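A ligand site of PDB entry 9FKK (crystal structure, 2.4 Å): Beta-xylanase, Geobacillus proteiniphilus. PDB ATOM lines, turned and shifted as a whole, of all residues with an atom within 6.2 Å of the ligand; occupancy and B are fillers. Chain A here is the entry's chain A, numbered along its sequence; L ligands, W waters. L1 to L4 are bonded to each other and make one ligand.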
ATOM      1  N   GLU A  44     -18.843 -16.034  -9.688  1.00  0.00           N
ATOM      2  CA  GLU A  44     -18.955 -16.376 -11.108  1.00  0.00           C
ATOM      3  C   GLU A  44     -17.585 -16.643 -11.728  1.00  0.00           C
ATOM      4  O   GLU A  44     -17.444 -17.539 -12.574  1.00  0.00           O
ATOM      5  CB  GLU A  44     -19.677 -15.250 -11.860  1.00  0.00           C
ATOM      6  CG  GLU A  44     -20.326 -15.714 -13.152  1.00  0.00           C
ATOM      7  CD  GLU A  44     -20.741 -14.559 -14.029  1.00  0.00           C
ATOM      8  OE1 GLU A  44     -20.982 -13.462 -13.490  1.00  0.00           O
ATOM      9  OE2 GLU A  44     -20.805 -14.747 -15.271  1.00  0.00           O
ATOM     10  N   ASN A  45     -16.565 -15.869 -11.345  1.00  0.00           N
ATOM     11  CA  ASN A  45     -15.238 -16.040 -11.943  1.00  0.00           C
ATOM     12  C   ASN A  45     -14.095 -15.921 -10.960  1.00  0.00           C
ATOM     13  O   ASN A  45     -13.023 -16.483 -11.232  1.00  0.00           O
ATOM     14  CB  ASN A  45     -15.016 -15.017 -13.075  1.00  0.00           C
ATOM     15  CG  ASN A  45     -15.753 -15.376 -14.353  1.00  0.00           C
ATOM     16  OD1 ASN A  45     -15.472 -16.413 -14.960  1.00  0.00           O
ATOM     17  ND2 ASN A  45     -16.699 -14.541 -14.757  1.00  0.00           N
ATOM     18  N   LYS A  48     -11.852 -18.919  -9.638  1.00  0.00           N
ATOM     19  CA  LYS A  48     -11.190 -19.855 -10.530  1.00  0.00           C
ATOM     20  C   LYS A  48      -9.678 -19.614 -10.483  1.00  0.00           C
ATOM     21  O   LYS A  48      -9.200 -18.597  -9.998  1.00  0.00           O
ATOM     22  CB  LYS A  48     -11.744 -19.715 -11.946  1.00  0.00           C
ATOM     23  CG  LYS A  48     -13.258 -19.684 -11.998  1.00  0.00           C
ATOM     24  CD  LYS A  48     -13.785 -19.522 -13.420  1.00  0.00           C
ATOM     25  CE  LYS A  48     -15.317 -19.642 -13.470  1.00  0.00           C
ATOM     26  NZ  LYS A  48     -15.849 -19.415 -14.853  1.00  0.00           N
ATOM     27  N   HIS A  81     -16.030 -22.139  -6.156  1.00  0.00           N
ATOM     28  CA  HIS A  81     -16.010 -22.526  -7.566  1.00  0.00           C
ATOM     29  C   HIS A  81     -14.833 -21.811  -8.224  1.00  0.00           C
ATOM     30  O   HIS A  81     -14.824 -20.578  -8.253  1.00  0.00           O
ATOM     31  CB  HIS A  81     -17.347 -22.145  -8.238  1.00  0.00           C
ATOM     32  CG  HIS A  81     -17.437 -22.501  -9.697  1.00  0.00           C
ATOM     33  ND1 HIS A  81     -17.758 -23.768 -10.136  1.00  0.00           N
ATOM     34  CD2 HIS A  81     -17.242 -21.753 -10.817  1.00  0.00           C
ATOM     35  CE1 HIS A  81     -17.743 -23.792 -11.458  1.00  0.00           C
ATOM     36  NE2 HIS A  81     -17.439 -22.580 -11.895  1.00  0.00           N
ATOM     37  N   THR A  82     -13.840 -22.548  -8.762  1.00  0.00           N
ATOM     38  CA  THR A  82     -13.703 -23.999  -8.795  1.00  0.00           C
ATOM     39  C   THR A  82     -12.178 -24.298  -8.783  1.00  0.00           C
ATOM     40  O   THR A  82     -11.396 -23.471  -9.257  1.00  0.00           O
ATOM     41  CB  THR A  82     -14.394 -24.628 -10.060  1.00  0.00           C
ATOM     42  OG1 THR A  82     -14.277 -26.058 -10.012  1.00  0.00           O
ATOM     43  CG2 THR A  82     -13.746 -24.151 -11.354  1.00  0.00           C
ATOM     44  N   TRP A  85      -9.905 -27.509 -13.343  1.00  0.00           N
ATOM     45  CA  TRP A  85     -10.741 -27.309 -14.518  1.00  0.00           C
ATOM     46  C   TRP A  85      -9.838 -27.131 -15.725  1.00  0.00           C
ATOM     47  O   TRP A  85      -8.774 -26.517 -15.610  1.00  0.00           O
ATOM     48  CB  TRP A  85     -11.644 -26.083 -14.344  1.00  0.00           C
ATOM     49  CG  TRP A  85     -12.737 -25.880 -15.394  1.00  0.00           C
ATOM     50  CD1 TRP A  85     -13.330 -26.841 -16.166  1.00  0.00           C
ATOM     51  CD2 TRP A  85     -13.371 -24.633 -15.752  1.00  0.00           C
ATOM     52  NE1 TRP A  85     -14.296 -26.274 -16.986  1.00  0.00           N
ATOM     53  CE2 TRP A  85     -14.329 -24.922 -16.752  1.00  0.00           C
ATOM     54  CE3 TRP A  85     -13.217 -23.311 -15.334  1.00  0.00           C
ATOM     55  CZ2 TRP A  85     -15.139 -23.930 -17.336  1.00  0.00           C
ATOM     56  CZ3 TRP A  85     -14.024 -22.331 -15.909  1.00  0.00           C
ATOM     57  CH2 TRP A  85     -14.975 -22.651 -16.893  1.00  0.00           C
ATOM     58  N   HIS A  86     -10.274 -27.628 -16.892  1.00  0.00           N
ATOM     59  CA  HIS A  86      -9.540 -27.423 -18.143  1.00  0.00           C
ATOM     60  C   HIS A  86      -9.585 -25.979 -18.648  1.00  0.00           C
ATOM     61  O   HIS A  86      -8.819 -25.640 -19.550  1.00  0.00           O
ATOM     62  CB  HIS A  86     -10.041 -28.371 -19.262  1.00  0.00           C
ATOM     63  CG  HIS A  86     -11.453 -28.100 -19.705  1.00  0.00           C
ATOM     64  ND1 HIS A  86     -12.557 -28.627 -19.070  1.00  0.00           N
ATOM     65  CD2 HIS A  86     -11.938 -27.346 -20.727  1.00  0.00           C
ATOM     66  CE1 HIS A  86     -13.659 -28.212 -19.669  1.00  0.00           C
ATOM     67  NE2 HIS A  86     -13.309 -27.429 -20.673  1.00  0.00           N
ATOM     68  N   ASN A  87     -10.445 -25.127 -18.084  1.00  0.00           N
ATOM     69  CA  ASN A  87     -10.519 -23.742 -18.523  1.00  0.00           C
ATOM     70  C   ASN A  87     -10.013 -22.778 -17.456  1.00  0.00           C
ATOM     71  O   ASN A  87      -9.880 -23.133 -16.276  1.00  0.00           O
ATOM     72  CB  ASN A  87     -11.954 -23.367 -18.908  1.00  0.00           C
ATOM     73  CG  ASN A  87     -12.313 -23.814 -20.311  1.00  0.00           C
ATOM     74  OD1 ASN A  87     -11.429 -23.979 -21.159  1.00  0.00           O
ATOM     75  ND2 ASN A  87     -13.606 -24.010 -20.571  1.00  0.00           N
ATOM     76  N   GLN A  88      -9.710 -21.556 -17.892  1.00  0.00           N
ATOM     77  CA  GLN A  88      -9.384 -20.451 -16.990  1.00  0.00           C
ATOM     78  C   GLN A  88      -8.323 -20.835 -15.959  1.00  0.00           C
ATOM     79  O   GLN A  88      -8.383 -20.475 -14.781  1.00  0.00           O
ATOM     80  CB  GLN A  88     -10.660 -19.922 -16.330  1.00  0.00           C
ATOM     81  CG  GLN A  88     -11.582 -19.261 -17.342  1.00  0.00           C
ATOM     82  CD  GLN A  88     -12.841 -18.687 -16.723  1.00  0.00           C
ATOM     83  OE1 GLN A  88     -13.897 -19.321 -16.738  1.00  0.00           O
ATOM     84  NE2 GLN A  88     -12.746 -17.484 -16.175  1.00  0.00           N
ATOM     85  N   ASN A 133     -14.213 -29.743 -12.181  1.00  0.00           N
ATOM     86  CA  ASN A 133     -15.216 -29.152 -13.052  1.00  0.00           C
ATOM     87  C   ASN A 133     -15.109 -29.760 -14.435  1.00  0.00           C
ATOM     88  O   ASN A 133     -14.039 -29.688 -15.063  1.00  0.00           O
ATOM     89  CB  ASN A 133     -15.059 -27.634 -13.137  1.00  0.00           C
ATOM     90  CG  ASN A 133     -16.371 -26.926 -13.472  1.00  0.00           C
ATOM     91  OD1 ASN A 133     -17.421 -27.295 -12.972  1.00  0.00           O
ATOM     92  ND2 ASN A 133     -16.300 -25.902 -14.321  1.00  0.00           N
ATOM     93  N   GLU A 134     -16.200 -30.384 -14.919  1.00  0.00           N
ATOM     94  CA  GLU A 134     -16.387 -30.690 -16.336  1.00  0.00           C
ATOM     95  C   GLU A 134     -15.302 -31.622 -16.898  1.00  0.00           C
ATOM     96  O   GLU A 134     -14.832 -31.435 -18.014  1.00  0.00           O
ATOM     97  CB  GLU A 134     -16.438 -29.421 -17.179  1.00  0.00           C
ATOM     98  CG  GLU A 134     -17.571 -28.464 -16.862  1.00  0.00           C
ATOM     99  CD  GLU A 134     -17.421 -27.136 -17.600  1.00  0.00           C
ATOM    100  OE1 GLU A 134     -16.493 -27.028 -18.434  1.00  0.00           O
ATOM    101  OE2 GLU A 134     -18.229 -26.205 -17.355  1.00  0.00           O
ATOM    102  N   ASP A 138     -17.908 -34.281 -23.246  1.00  0.00           N
ATOM    103  CA  ASP A 138     -19.227 -33.805 -23.674  1.00  0.00           C
ATOM    104  C   ASP A 138     -19.696 -34.470 -24.973  1.00  0.00           C
ATOM    105  O   ASP A 138     -20.894 -34.416 -25.267  1.00  0.00           O
ATOM    106  CB  ASP A 138     -19.218 -32.275 -23.841  1.00  0.00           C
ATOM    107  CG  ASP A 138     -20.626 -31.662 -23.907  1.00  0.00           C
ATOM    108  OD1 ASP A 138     -21.504 -31.990 -23.066  1.00  0.00           O
ATOM    109  OD2 ASP A 138     -20.867 -30.829 -24.813  1.00  0.00           O
ATOM    110  N   ARG A 145     -12.849 -36.010 -21.028  1.00  0.00           N
ATOM    111  CA  ARG A 145     -12.316 -34.911 -21.801  1.00  0.00           C
ATOM    112  C   ARG A 145     -10.781 -34.981 -21.760  1.00  0.00           C
ATOM    113  O   ARG A 145     -10.217 -35.503 -20.801  1.00  0.00           O
ATOM    114  CB  ARG A 145     -12.836 -33.604 -21.195  1.00  0.00           C
ATOM    115  CG  ARG A 145     -12.666 -32.358 -21.998  1.00  0.00           C
ATOM    116  CD  ARG A 145     -13.025 -31.162 -21.135  1.00  0.00           C
ATOM    117  NE  ARG A 145     -14.451 -31.105 -20.822  1.00  0.00           N
ATOM    118  CZ  ARG A 145     -15.350 -30.518 -21.618  1.00  0.00           C
ATOM    119  NH1 ARG A 145     -14.967 -29.970 -22.758  1.00  0.00           N
ATOM    120  NH2 ARG A 145     -16.631 -30.488 -21.276  1.00  0.00           N
ATOM    121  N   ASN A 177     -18.710 -31.298 -10.598  1.00  0.00           N
ATOM    122  CA  ASN A 177     -19.620 -30.319 -11.207  1.00  0.00           C
ATOM    123  C   ASN A 177     -19.563 -30.389 -12.732  1.00  0.00           C
ATOM    124  O   ASN A 177     -18.476 -30.391 -13.320  1.00  0.00           O
ATOM    125  CB  ASN A 177     -19.240 -28.902 -10.738  1.00  0.00           C
ATOM    126  CG  ASN A 177     -20.344 -27.862 -10.974  1.00  0.00           C
ATOM    127  OD1 ASN A 177     -21.489 -28.043 -10.576  1.00  0.00           O
ATOM    128  ND2 ASN A 177     -19.977 -26.744 -11.626  1.00  0.00           N
ATOM    129  N   TYR A 179     -22.072 -29.927 -16.750  1.00  0.00           N
ATOM    130  CA  TYR A 179     -23.199 -29.471 -17.547  1.00  0.00           C
ATOM    131  C   TYR A 179     -23.615 -30.560 -18.547  1.00  0.00           C
ATOM    132  O   TYR A 179     -22.901 -31.537 -18.769  1.00  0.00           O
ATOM    133  CB  TYR A 179     -22.853 -28.182 -18.302  1.00  0.00           C
ATOM    134  CG  TYR A 179     -21.780 -28.353 -19.371  1.00  0.00           C
ATOM    135  CD1 TYR A 179     -20.408 -28.301 -19.053  1.00  0.00           C
ATOM    136  CD2 TYR A 179     -22.134 -28.587 -20.692  1.00  0.00           C
ATOM    137  CE1 TYR A 179     -19.431 -28.474 -20.054  1.00  0.00           C
ATOM    138  CE2 TYR A 179     -21.176 -28.752 -21.687  1.00  0.00           C
ATOM    139  CZ  TYR A 179     -19.836 -28.691 -21.369  1.00  0.00           C
ATOM    140  OH  TYR A 179     -18.915 -28.866 -22.386  1.00  0.00           O
ATOM    141  N   ASN A 180     -24.763 -30.334 -19.183  1.00  0.00           N
ATOM    142  CA  ASN A 180     -25.419 -31.362 -20.016  1.00  0.00           C
ATOM    143  C   ASN A 180     -25.562 -32.673 -19.247  1.00  0.00           C
ATOM    144  O   ASN A 180     -25.601 -33.760 -19.822  1.00  0.00           O
ATOM    145  CB  ASN A 180     -24.686 -31.561 -21.348  1.00  0.00           C
ATOM    146  CG  ASN A 180     -24.876 -30.387 -22.307  1.00  0.00           C
ATOM    147  OD1 ASN A 180     -24.111 -30.233 -23.269  1.00  0.00           O
ATOM    148  ND2 ASN A 180     -25.897 -29.556 -22.075  1.00  0.00           N
ATOM    149  N   PHE A 183     -28.426 -35.288 -20.291  1.00  0.00           N
ATOM    150  CA  PHE A 183     -28.444 -36.048 -21.528  1.00  0.00           C
ATOM    151  C   PHE A 183     -27.968 -37.468 -21.226  1.00  0.00           C
ATOM    152  O   PHE A 183     -26.905 -37.644 -20.624  1.00  0.00           O
ATOM    153  CB  PHE A 183     -27.585 -35.383 -22.603  1.00  0.00           C
ATOM    154  CG  PHE A 183     -28.071 -33.994 -22.989  1.00  0.00           C
ATOM    155  CD1 PHE A 183     -29.407 -33.639 -22.788  1.00  0.00           C
ATOM    156  CD2 PHE A 183     -27.214 -33.056 -23.536  1.00  0.00           C
ATOM    157  CE1 PHE A 183     -29.869 -32.366 -23.119  1.00  0.00           C
ATOM    158  CE2 PHE A 183     -27.669 -31.781 -23.879  1.00  0.00           C
ATOM    159  CZ  PHE A 183     -28.992 -31.436 -23.672  1.00  0.00           C
ATOM    160  N   GLN A 210     -25.143 -28.411 -13.246  1.00  0.00           N
ATOM    161  CA  GLN A 210     -25.057 -27.021 -13.667  1.00  0.00           C
ATOM    162  C   GLN A 210     -26.403 -26.497 -14.177  1.00  0.00           C
ATOM    163  O   GLN A 210     -26.806 -25.375 -13.841  1.00  0.00           O
ATOM    164  CB  GLN A 210     -23.981 -26.839 -14.735  1.00  0.00           C
ATOM    165  CG  GLN A 210     -22.548 -26.827 -14.208  1.00  0.00           C
ATOM    166  CD  GLN A 210     -21.562 -26.468 -15.285  1.00  0.00           C
ATOM    167  OE1 GLN A 210     -21.910 -25.784 -16.248  1.00  0.00           O
ATOM    168  NE2 GLN A 210     -20.334 -26.936 -15.154  1.00  0.00           N
ATOM    169  N   HIS A 212     -27.530 -25.630 -17.323  1.00  0.00           N
ATOM    170  CA  HIS A 212     -27.591 -24.573 -18.341  1.00  0.00           C
ATOM    171  C   HIS A 212     -28.534 -25.083 -19.430  1.00  0.00           C
ATOM    172  O   HIS A 212     -28.134 -25.699 -20.426  1.00  0.00           O
ATOM    173  CB  HIS A 212     -26.195 -24.223 -18.877  1.00  0.00           C
ATOM    174  CG  HIS A 212     -25.328 -23.537 -17.865  1.00  0.00           C
ATOM    175  ND1 HIS A 212     -25.679 -22.354 -17.245  1.00  0.00           N
ATOM    176  CD2 HIS A 212     -24.121 -23.877 -17.351  1.00  0.00           C
ATOM    177  CE1 HIS A 212     -24.729 -21.997 -16.403  1.00  0.00           C
ATOM    178  NE2 HIS A 212     -23.774 -22.912 -16.447  1.00  0.00           N
ATOM    179  N   PHE A 249     -29.772 -24.638 -28.918  1.00  0.00           N
ATOM    180  CA  PHE A 249     -28.366 -24.697 -29.309  1.00  0.00           C
ATOM    181  C   PHE A 249     -28.174 -24.372 -30.792  1.00  0.00           C
ATOM    182  O   PHE A 249     -27.228 -23.661 -31.156  1.00  0.00           O
ATOM    183  CB  PHE A 249     -27.816 -26.085 -28.993  1.00  0.00           C
ATOM    184  CG  PHE A 249     -26.421 -26.296 -29.468  1.00  0.00           C
ATOM    185  CD1 PHE A 249     -25.337 -25.799 -28.744  1.00  0.00           C
ATOM    186  CD2 PHE A 249     -26.168 -27.009 -30.652  1.00  0.00           C
ATOM    187  CE1 PHE A 249     -24.041 -25.988 -29.190  1.00  0.00           C
ATOM    188  CE2 PHE A 249     -24.880 -27.218 -31.097  1.00  0.00           C
ATOM    189  CZ  PHE A 249     -23.807 -26.702 -30.368  1.00  0.00           C
ATOM    190  N   TRP A 291     -27.140 -19.003 -12.222  1.00  0.00           N
ATOM    191  CA  TRP A 291     -25.903 -18.377 -12.687  1.00  0.00           C
ATOM    192  C   TRP A 291     -26.113 -16.884 -12.984  1.00  0.00           C
ATOM    193  O   TRP A 291     -25.971 -16.419 -14.116  1.00  0.00           O
ATOM    194  CB  TRP A 291     -25.363 -19.114 -13.891  1.00  0.00           C
ATOM    195  CG  TRP A 291     -23.867 -19.082 -13.964  1.00  0.00           C
ATOM    196  CD1 TRP A 291     -23.101 -18.561 -14.963  1.00  0.00           C
ATOM    197  CD2 TRP A 291     -22.953 -19.600 -12.977  1.00  0.00           C
ATOM    198  NE1 TRP A 291     -21.761 -18.728 -14.678  1.00  0.00           N
ATOM    199  CE2 TRP A 291     -21.641 -19.360 -13.469  1.00  0.00           C
ATOM    200  CE3 TRP A 291     -23.106 -20.237 -11.744  1.00  0.00           C
ATOM    201  CZ2 TRP A 291     -20.490 -19.725 -12.753  1.00  0.00           C
ATOM    202  CZ3 TRP A 291     -21.965 -20.613 -11.027  1.00  0.00           C
ATOM    203  CH2 TRP A 291     -20.671 -20.351 -11.543  1.00  0.00           C
ATOM    204  N   HIS A 297     -27.544  -8.925 -16.088  1.00  0.00           N
ATOM    205  CA  HIS A 297     -26.230  -9.555 -16.185  1.00  0.00           C
ATOM    206  C   HIS A 297     -26.383 -11.061 -16.382  1.00  0.00           C
ATOM    207  O   HIS A 297     -26.923 -11.738 -15.513  1.00  0.00           O
ATOM    208  CB  HIS A 297     -25.373  -9.296 -14.951  1.00  0.00           C
ATOM    209  CG  HIS A 297     -24.072 -10.036 -14.971  1.00  0.00           C
ATOM    210  ND1 HIS A 297     -22.965  -9.573 -15.655  1.00  0.00           N
ATOM    211  CD2 HIS A 297     -23.702 -11.217 -14.417  1.00  0.00           C
ATOM    212  CE1 HIS A 297     -21.972 -10.427 -15.505  1.00  0.00           C
ATOM    213  NE2 HIS A 297     -22.394 -11.428 -14.753  1.00  0.00           N
ATOM    214  N   TRP A 299     -23.971 -14.366 -18.486  1.00  0.00           N
ATOM    215  CA  TRP A 299     -22.963 -14.818 -19.418  1.00  0.00           C
ATOM    216  C   TRP A 299     -23.561 -15.255 -20.742  1.00  0.00           C
ATOM    217  O   TRP A 299     -22.828 -15.350 -21.740  1.00  0.00           O
ATOM    218  CB  TRP A 299     -22.159 -15.972 -18.827  1.00  0.00           C
ATOM    219  CG  TRP A 299     -22.920 -17.286 -18.761  1.00  0.00           C
ATOM    220  CD1 TRP A 299     -24.113 -17.524 -18.136  1.00  0.00           C
ATOM    221  CD2 TRP A 299     -22.524 -18.531 -19.348  1.00  0.00           C
ATOM    222  NE1 TRP A 299     -24.476 -18.845 -18.287  1.00  0.00           N
ATOM    223  CE2 TRP A 299     -23.515 -19.482 -19.026  1.00  0.00           C
ATOM    224  CE3 TRP A 299     -21.408 -18.937 -20.098  1.00  0.00           C
ATOM    225  CZ2 TRP A 299     -23.441 -20.811 -19.447  1.00  0.00           C
ATOM    226  CZ3 TRP A 299     -21.332 -20.258 -20.508  1.00  0.00           C
ATOM    227  CH2 TRP A 299     -22.345 -21.179 -20.187  1.00  0.00           C
ATOM    228  N   PHE A 303     -22.428 -15.964 -24.750  1.00  0.00           N
ATOM    229  CA  PHE A 303     -22.207 -17.386 -25.002  1.00  0.00           C
ATOM    230  C   PHE A 303     -23.537 -18.062 -25.309  1.00  0.00           C
ATOM    231  O   PHE A 303     -24.524 -17.851 -24.562  1.00  0.00           O
ATOM    232  CB  PHE A 303     -21.525 -18.068 -23.810  1.00  0.00           C
ATOM    233  CG  PHE A 303     -21.179 -19.514 -24.068  1.00  0.00           C
ATOM    234  CD1 PHE A 303     -20.000 -19.856 -24.724  1.00  0.00           C
ATOM    235  CD2 PHE A 303     -22.049 -20.524 -23.702  1.00  0.00           C
ATOM    236  CE1 PHE A 303     -19.685 -21.182 -24.983  1.00  0.00           C
ATOM    237  CE2 PHE A 303     -21.743 -21.850 -23.958  1.00  0.00           C
ATOM    238  CZ  PHE A 303     -20.560 -22.185 -24.594  1.00  0.00           C
HETATM  239  C1  LIG L   1     -24.251 -27.541 -24.899  1.00  0.00           C
HETATM  240  C2  LIG L   1     -24.837 -26.489 -23.923  1.00  0.00           C
HETATM  241  C3  LIG L   1     -23.863 -25.422 -23.395  1.00  0.00           C
HETATM  242  C4  LIG L   1     -22.430 -25.953 -23.327  1.00  0.00           C
HETATM  243  C5  LIG L   1     -22.051 -26.466 -24.715  1.00  0.00           C
HETATM  244  O1  LIG L   1     -26.048 -25.906 -24.454  1.00  0.00           O
HETATM  245  O2  LIG L   1     -24.262 -25.003 -22.073  1.00  0.00           O
HETATM  246  O3  LIG L   1     -21.501 -24.936 -22.906  1.00  0.00           O
HETATM  247  O4  LIG L   1     -22.825 -27.641 -24.997  1.00  0.00           O
HETATM  248  F1  LIG L   1     -24.917 -27.684 -26.082  1.00  0.00           F
HETATM  249  C1  LG2 L   2     -20.783 -25.178 -21.681  1.00  0.00           C
HETATM  250  C2  LG2 L   2     -19.473 -24.370 -21.752  1.00  0.00           C
HETATM  251  C3  LG2 L   2     -18.751 -24.343 -20.398  1.00  0.00           C
HETATM  252  C4  LG2 L   2     -19.714 -23.782 -19.343  1.00  0.00           C
HETATM  253  C5  LG2 L   2     -20.903 -24.757 -19.259  1.00  0.00           C
HETATM  254  O1  LG2 L   2     -18.619 -24.900 -22.774  1.00  0.00           O
HETATM  255  O2  LG2 L   2     -17.518 -23.610 -20.465  1.00  0.00           O
HETATM  256  O3  LG2 L   2     -19.021 -23.532 -18.105  1.00  0.00           O
HETATM  257  O4  LG2 L   2     -21.591 -24.863 -20.516  1.00  0.00           O
HETATM  258  C1  LG3 L   3     -19.774 -23.394 -16.868  1.00  0.00           C
HETATM  259  C2  LG3 L   3     -18.788 -23.172 -15.705  1.00  0.00           C
HETATM  260  C3  LG3 L   3     -18.802 -21.739 -15.186  1.00  0.00           C
HETATM  261  C4  LG3 L   3     -18.909 -20.788 -16.368  1.00  0.00           C
HETATM  262  C5  LG3 L   3     -20.240 -21.016 -17.080  1.00  0.00           C
HETATM  263  O1  LG3 L   3     -19.064 -24.071 -14.619  1.00  0.00           O
HETATM  264  O2  LG3 L   3     -17.612 -21.500 -14.455  1.00  0.00           O
HETATM  265  O3  LG3 L   3     -18.777 -19.424 -15.981  1.00  0.00           O
HETATM  266  O4  LG3 L   3     -20.747 -22.346 -16.847  1.00  0.00           O
HETATM  267  C1  LG4 L   4     -18.638 -18.585 -17.129  1.00  0.00           C
HETATM  268  C2  LG4 L   4     -18.690 -17.137 -16.671  1.00  0.00           C
HETATM  269  C3  LG4 L   4     -18.211 -16.242 -17.815  1.00  0.00           C
HETATM  270  C4  LG4 L   4     -16.739 -16.526 -18.141  1.00  0.00           C
HETATM  271  C5  LG4 L   4     -16.359 -17.985 -17.899  1.00  0.00           C
HETATM  272  O1  LG4 L   4     -20.037 -16.846 -16.264  1.00  0.00           O
HETATM  273  O2  LG4 L   4     -18.327 -14.884 -17.389  1.00  0.00           O
HETATM  274  O3  LG4 L   4     -16.387 -16.109 -19.473  1.00  0.00           O
HETATM  275  O4  LG4 L   4     -17.452 -18.918 -17.870  1.00  0.00           O
HETATM  276  O   HOH W   1     -24.877 -22.458 -22.593  1.00  0.00           O
HETATM  277  O   HOH W   2     -27.633 -29.387 -27.194  1.00  0.00           O
HETATM  278  O   HOH W   3     -29.079 -27.311 -24.844  1.00  0.00           O
HETATM  279  O   HOH W   4     -20.639 -12.819 -17.332  1.00  0.00           O
HETATM  280  O   HOH W   5     -18.102 -16.925 -22.063  1.00  0.00           O
HETATM  281  O   HOH W   6     -25.854 -26.787 -21.225  1.00  0.00           O
HETATM  282  O   HOH W   7     -28.709 -24.667 -23.179  1.00  0.00           O
HETATM  283  O   HOH W   8     -25.206 -23.175 -25.449  1.00  0.00           O
HETATM  284  O   HOH W   9     -16.039 -26.115 -22.021  1.00  0.00           O
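The side-chain carboxylate (OE2) of Glu 44 is in hydrogen-bond range of an oxygen (O1) of LG4 L4, 2.4 Å away. NZ of Lys 48 is in hydrogen-bond range of O2 of LG3 L3 (2.8 Å). An oxygen (O2) of LG3 L3 sits at hydrogen-bond distance from a ring nitrogen (NE2) of His 81 (2.8 Å). The indole nitrogen (NE1) of Trp 291 lies within hydrogen-bond range of an oxygen (O1) of LG4 L4 (3.0 Å). An oxygen (O4) of LG3 L3 is in hydrogen-bond range of a ring nitrogen (NE2) of His 212 (3.1 Å). ND2 of Asn 45 is in hydrogen-bond range of O2 of LG4 L4 (3.1 Å). The side-chain amide oxygen of Asn 180 lies close to an oxygen (O4) of LIG L1 (3.4 Å). The side-chain amide nitrogen of Gln 210 sits at hydrogen-bond distance from an oxygen (O1) of LG3 L3. The side-chain amide nitrogen (ND2) of Asn 133 is in hydrogen-bond range of an oxygen (O1) of LG3 L3.
The side-chain amide oxygen of Gln 88 is in hydrogen-bond range of the side-chain amino group of Lys 48 (2.7 Å). The side-chain amide nitrogen of Gln 210 is in hydrogen-bond range of the side-chain carboxylate of Glu 134 (3.1 Å). The indole nitrogen (NE1) of Trp 85 is in hydrogen-bond range of the side-chain carboxylate (OE1) of Glu 134 (2.7 Å). N of Glu 134 lies within hydrogen-bond range of O of Asn 177, 2.8 Å away. NE2 of Gln 88 sits at hydrogen-bond distance from OD1 of Asn 45, 3.2 Å away. A ring nitrogen (NE2) of His 212 lies close to the side-chain amide oxygen (OE1) of Gln 210. The side-chain amide oxygen (OD1) of Asn 180 sits close to the side-chain carboxylate (OD1) of Asp 138, at 3.2 Å. The side-chain amide oxygen of Asn 133 lies within hydrogen-bond range of the side-chain amide nitrogen of Asn 177, at 2.9 Å.
The side-chain carboxylate of Glu 134 lies close to an oxygen (O3) of LG2 L2 (2.9 Å). Residues that only touch the ligand: Gln 88, Phe 303, Phe 249, Trp 299, Tyr 179, Asp 138, Trp 85 and Asn 87. Hydrophobic or aromatic side chains within 4 Å of the ligand: His 81, Trp 85, Tyr 179, His 212, Phe 249, Trp 291, Trp 299 and Phe 303. Within 4 Å of the ligand: Glu 44, Asn 45, Lys 48, His 81, Trp 85, Asn 87, Gln 88, Asn 133, Glu 134, Asp 138, Tyr 179, Asn 180, Gln 210, His 212, Phe 249, Trp 291, Trp 299 and Phe 303.
Water W6 lies within hydrogen-bond range of O2 of LIG L1, O of His 212 and ND2 of Asn 180. Water W9 bridges an oxygen (O1) of LG2 L2 (2.9 Å) and a ring nitrogen (NE2) of His 86 (3.3 Å). Water W4 lies within hydrogen-bond range of the side-chain carboxylate of Glu 44 (2.8 Å), an oxygen (O2) of LG4 L4 (3.1 Å) and a ring nitrogen (NE2) of His 297 (3.4 Å). Water W7 bridges the backbone carbonyl oxygen of His 212 (3.0 Å) and an oxygen (O1) of LIG L1 (3.2 Å).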
